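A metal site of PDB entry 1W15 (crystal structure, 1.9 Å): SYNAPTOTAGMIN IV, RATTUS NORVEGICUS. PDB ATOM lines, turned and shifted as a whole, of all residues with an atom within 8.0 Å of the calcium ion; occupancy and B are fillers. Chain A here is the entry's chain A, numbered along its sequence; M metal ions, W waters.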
ATOM      1  N   LEU A  50     -26.023 -13.262 -37.967  1.00  0.00           N
ATOM      2  CA  LEU A  50     -26.871 -13.495 -36.785  1.00  0.00           C
ATOM      3  C   LEU A  50     -26.073 -13.590 -35.475  1.00  0.00           C
ATOM      4  O   LEU A  50     -24.907 -14.008 -35.447  1.00  0.00           O
ATOM      5  CB  LEU A  50     -27.771 -14.723 -36.981  1.00  0.00           C
ATOM      6  CG  LEU A  50     -29.015 -14.554 -37.862  1.00  0.00           C
ATOM      7  CD1 LEU A  50     -29.555 -15.896 -38.352  1.00  0.00           C
ATOM      8  CD2 LEU A  50     -30.089 -13.805 -37.097  1.00  0.00           C
ATOM      9  N   SER A  51     -26.703 -13.168 -34.406  1.00  0.00           N
ATOM     10  CA  SER A  51     -26.014 -13.109 -33.136  1.00  0.00           C
ATOM     11  C   SER A  51     -26.129 -14.467 -32.446  1.00  0.00           C
ATOM     12  O   SER A  51     -26.916 -15.334 -32.884  1.00  0.00           O
ATOM     13  CB  SER A  51     -26.560 -11.957 -32.305  1.00  0.00           C
ATOM     14  OG  SER A  51     -27.881 -12.251 -31.815  1.00  0.00           O
ATOM     15  N   ASP A  52     -25.323 -14.652 -31.405  1.00  0.00           N
ATOM     16  CA  ASP A  52     -25.331 -15.845 -30.557  1.00  0.00           C
ATOM     17  C   ASP A  52     -25.688 -15.371 -29.170  1.00  0.00           C
ATOM     18  O   ASP A  52     -24.779 -15.173 -28.363  1.00  0.00           O
ATOM     19  CB  ASP A  52     -23.930 -16.458 -30.541  1.00  0.00           C
ATOM     20  CG  ASP A  52     -23.469 -16.807 -31.928  1.00  0.00           C
ATOM     21  OD1 ASP A  52     -24.166 -17.558 -32.613  1.00  0.00           O
ATOM     22  OD2 ASP A  52     -22.430 -16.353 -32.431  1.00  0.00           O
ATOM     23  N   PRO A  53     -26.984 -15.113 -28.905  1.00  0.00           N
ATOM     24  CA  PRO A  53     -27.378 -14.440 -27.664  1.00  0.00           C
ATOM     25  C   PRO A  53     -27.302 -15.252 -26.370  1.00  0.00           C
ATOM     26  O   PRO A  53     -27.567 -16.436 -26.378  1.00  0.00           O
ATOM     27  CB  PRO A  53     -28.829 -13.994 -27.916  1.00  0.00           C
ATOM     28  CG  PRO A  53     -29.338 -14.979 -29.005  1.00  0.00           C
ATOM     29  CD  PRO A  53     -28.141 -15.344 -29.808  1.00  0.00           C
ATOM     30  N   VAL A  73     -25.734 -19.843 -23.882  1.00  0.00           N
ATOM     31  CA  VAL A  73     -25.904 -19.084 -25.117  1.00  0.00           C
ATOM     32  C   VAL A  73     -26.630 -19.908 -26.174  1.00  0.00           C
ATOM     33  O   VAL A  73     -26.396 -21.102 -26.342  1.00  0.00           O
ATOM     34  CB  VAL A  73     -24.548 -18.597 -25.650  1.00  0.00           C
ATOM     35  CG1 VAL A  73     -23.412 -19.179 -24.834  1.00  0.00           C
ATOM     36  CG2 VAL A  73     -24.383 -18.971 -27.111  1.00  0.00           C
ATOM     37  N   LYS A  74     -27.509 -19.216 -26.913  1.00  0.00           N
ATOM     38  CA  LYS A  74     -28.164 -19.808 -28.076  1.00  0.00           C
ATOM     39  C   LYS A  74     -27.417 -19.349 -29.346  1.00  0.00           C
ATOM     40  O   LYS A  74     -27.104 -18.171 -29.484  1.00  0.00           O
ATOM     41  CB  LYS A  74     -29.639 -19.422 -28.051  1.00  0.00           C
ATOM     42  CG  LYS A  74     -30.334 -19.951 -26.781  1.00  0.00           C
ATOM     43  CD  LYS A  74     -30.164 -21.482 -26.704  1.00  0.00           C
ATOM     44  CE  LYS A  74     -30.978 -22.191 -25.596  1.00  0.00           C
ATOM     45  NZ  LYS A  74     -30.234 -22.252 -24.297  1.00  0.00           N
ATOM     46  N   LYS A  75     -27.063 -20.272 -30.235  1.00  0.00           N
ATOM     47  CA  LYS A  75     -26.196 -19.929 -31.387  1.00  0.00           C
ATOM     48  C   LYS A  75     -26.943 -19.400 -32.637  1.00  0.00           C
ATOM     49  O   LYS A  75     -27.973 -19.963 -33.044  1.00  0.00           O
ATOM     50  CB  LYS A  75     -25.319 -21.132 -31.789  1.00  0.00           C
ATOM     51  CG  LYS A  75     -24.183 -21.434 -30.802  1.00  0.00           C
ATOM     52  CD  LYS A  75     -23.517 -22.785 -31.173  1.00  0.00           C
ATOM     53  CE  LYS A  75     -22.007 -22.790 -30.917  1.00  0.00           C
ATOM     54  NZ  LYS A  75     -21.383 -24.064 -31.399  1.00  0.00           N
ATOM     55  N   CYS A  76     -26.408 -18.318 -33.208  1.00  0.00           N
ATOM     56  CA  CYS A  76     -26.798 -17.790 -34.537  1.00  0.00           C
ATOM     57  C   CYS A  76     -28.316 -17.685 -34.796  1.00  0.00           C
ATOM     58  O   CYS A  76     -28.875 -18.433 -35.648  1.00  0.00           O
ATOM     59  CB  CYS A  76     -26.098 -18.611 -35.630  1.00  0.00           C
ATOM     60  SG  CYS A  76     -26.260 -17.927 -37.304  1.00  0.00           S
ATOM     61  N   LEU A 105     -26.571 -10.154 -24.747  1.00  0.00           N
ATOM     62  CA  LEU A 105     -25.205 -10.025 -25.265  1.00  0.00           C
ATOM     63  C   LEU A 105     -25.002 -11.025 -26.356  1.00  0.00           C
ATOM     64  O   LEU A 105     -25.631 -12.090 -26.358  1.00  0.00           O
ATOM     65  CB  LEU A 105     -24.198 -10.319 -24.137  1.00  0.00           C
ATOM     66  CG  LEU A 105     -24.283  -9.288 -22.982  1.00  0.00           C
ATOM     67  CD1 LEU A 105     -24.479  -9.925 -21.627  1.00  0.00           C
ATOM     68  CD2 LEU A 105     -22.942  -8.547 -23.077  1.00  0.00           C
ATOM     69  N   ASP A 106     -24.081 -10.706 -27.267  1.00  0.00           N
ATOM     70  CA  ASP A 106     -23.764 -11.604 -28.351  1.00  0.00           C
ATOM     71  C   ASP A 106     -22.431 -12.259 -27.976  1.00  0.00           C
ATOM     72  O   ASP A 106     -21.425 -11.561 -27.771  1.00  0.00           O
ATOM     73  CB  ASP A 106     -23.637 -10.793 -29.631  1.00  0.00           C
ATOM     74  CG  ASP A 106     -23.160 -11.595 -30.796  1.00  0.00           C
ATOM     75  OD1 ASP A 106     -23.464 -12.798 -30.919  1.00  0.00           O
ATOM     76  OD2 ASP A 106     -22.428 -11.091 -31.646  1.00  0.00           O
ATOM     77  N   SER A 107     -22.442 -13.585 -27.842  1.00  0.00           N
ATOM     78  CA  SER A 107     -21.222 -14.300 -27.540  1.00  0.00           C
ATOM     79  C   SER A 107     -20.327 -14.363 -28.766  1.00  0.00           C
ATOM     80  O   SER A 107     -20.737 -14.826 -29.829  1.00  0.00           O
ATOM     81  CB  SER A 107     -21.571 -15.700 -27.017  1.00  0.00           C
ATOM     82  OG  SER A 107     -20.417 -16.480 -26.934  1.00  0.00           O
ATOM     83  N   GLU A 108     -19.102 -13.858 -28.633  1.00  0.00           N
ATOM     84  CA  GLU A 108     -18.205 -13.806 -29.788  1.00  0.00           C
ATOM     85  C   GLU A 108     -16.812 -14.156 -29.288  1.00  0.00           C
ATOM     86  O   GLU A 108     -16.275 -13.443 -28.436  1.00  0.00           O
ATOM     87  CB  GLU A 108     -18.194 -12.403 -30.408  1.00  0.00           C
ATOM     88  CG  GLU A 108     -17.343 -12.324 -31.681  1.00  0.00           C
ATOM     89  CD  GLU A 108     -18.074 -12.834 -32.917  1.00  0.00           C
ATOM     90  OE1 GLU A 108     -19.312 -12.858 -32.901  1.00  0.00           O
ATOM     91  OE2 GLU A 108     -17.426 -13.210 -33.907  1.00  0.00           O
ATOM     92  N   ARG A 109     -16.202 -15.197 -29.809  1.00  0.00           N
ATOM     93  CA  ARG A 109     -14.852 -15.558 -29.388  1.00  0.00           C
ATOM     94  C   ARG A 109     -13.851 -14.526 -29.892  1.00  0.00           C
ATOM     95  O   ARG A 109     -13.872 -14.146 -31.072  1.00  0.00           O
ATOM     96  CB  ARG A 109     -14.456 -16.960 -29.926  1.00  0.00           C
ATOM     97  CG  ARG A 109     -15.340 -18.114 -29.377  1.00  0.00           C
ATOM     98  CD  ARG A 109     -14.974 -19.513 -29.990  1.00  0.00           C
ATOM     99  NE  ARG A 109     -16.069 -20.517 -30.049  1.00  0.00           N
ATOM    100  CZ  ARG A 109     -17.322 -20.436 -29.526  1.00  0.00           C
ATOM    101  NH1 ARG A 109     -17.739 -19.368 -28.852  1.00  0.00           N
ATOM    102  NH2 ARG A 109     -18.171 -21.462 -29.698  1.00  0.00           N
ATOM    103  N   SER A 111     -13.102 -11.387 -28.869  1.00  0.00           N
ATOM    104  CA  SER A 111     -13.472  -9.957 -28.649  1.00  0.00           C
ATOM    105  C   SER A 111     -14.436  -9.792 -27.499  1.00  0.00           C
ATOM    106  O   SER A 111     -15.072 -10.750 -27.093  1.00  0.00           O
ATOM    107  CB  SER A 111     -14.130  -9.323 -29.873  1.00  0.00           C
ATOM    108  OG  SER A 111     -15.256 -10.116 -30.257  1.00  0.00           O
ATOM    109  N   ASN A 113     -17.810  -9.309 -25.746  1.00  0.00           N
ATOM    110  CA  ASN A 113     -19.172  -9.609 -26.197  1.00  0.00           C
ATOM    111  C   ASN A 113     -19.989  -8.310 -26.192  1.00  0.00           C
ATOM    112  O   ASN A 113     -19.973  -7.571 -25.223  1.00  0.00           O
ATOM    113  CB  ASN A 113     -19.836 -10.618 -25.254  1.00  0.00           C
ATOM    114  CG  ASN A 113     -19.183 -11.994 -25.357  1.00  0.00           C
ATOM    115  OD1 ASN A 113     -18.436 -12.271 -26.277  1.00  0.00           O
ATOM    116  ND2 ASN A 113     -19.467 -12.850 -24.392  1.00  0.00           N
ATOM    117  N   GLU A 114     -20.680  -8.024 -27.283  1.00  0.00           N
ATOM    118  CA  GLU A 114     -21.394  -6.752 -27.418  1.00  0.00           C
ATOM    119  C   GLU A 114     -22.750  -6.842 -26.765  1.00  0.00           C
ATOM    120  O   GLU A 114     -23.375  -7.913 -26.759  1.00  0.00           O
ATOM    121  CB  GLU A 114     -21.551  -6.449 -28.907  1.00  0.00           C
ATOM    122  CG  GLU A 114     -22.507  -5.293 -29.205  1.00  0.00           C
ATOM    123  CD  GLU A 114     -22.159  -4.640 -30.544  1.00  0.00           C
ATOM    124  OE1 GLU A 114     -21.455  -5.300 -31.322  1.00  0.00           O
ATOM    125  OE2 GLU A 114     -22.547  -3.470 -30.789  1.00  0.00           O
ATOM    126  N   ILE A 116     -26.439  -6.345 -26.902  1.00  0.00           N
ATOM    127  CA  ILE A 116     -27.422  -6.217 -27.975  1.00  0.00           C
ATOM    128  C   ILE A 116     -28.575  -5.323 -27.483  1.00  0.00           C
ATOM    129  O   ILE A 116     -29.129  -4.502 -28.239  1.00  0.00           O
ATOM    130  CB  ILE A 116     -28.005  -7.614 -28.311  1.00  0.00           C
ATOM    131  CG1 ILE A 116     -26.972  -8.538 -28.974  1.00  0.00           C
ATOM    132  CG2 ILE A 116     -29.273  -7.517 -29.191  1.00  0.00           C
ATOM    133  CD1 ILE A 116     -27.509 -10.012 -29.091  1.00  0.00           C
HETATM  134 CA    CA M   1     -21.511 -14.045 -32.254  1.00  0.00          CA
HETATM  135  O   HOH W   1     -20.336 -14.175 -34.736  1.00  0.00           O
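Within 4 Å of the calcium ion: Asp 52, Asp 106, Ser 107 and Glu 108.
O of Asp 106 lies close to OD1 of Asn 113 (3.4 Å). N of Asp 106 is in hydrogen-bond range of O of Glu 114, 2.9 Å away. The side-chain amide oxygen (OD1) of Asn 113 lies within hydrogen-bond range of the backbone NH (N) of Glu 108. The side-chain carboxylate (OD1) of Asp 52 lies within hydrogen-bond range of the backbone NH (N) of Cys 76.
The calcium ion is bound by OD2 of Asp 52 (2.5 Å), OE1 of Glu 108 (2.6 Å), O of Ser 107 (2.7 Å), OD1 of Asp 106 (2.7 Å) and water W1 (2.7 Å).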
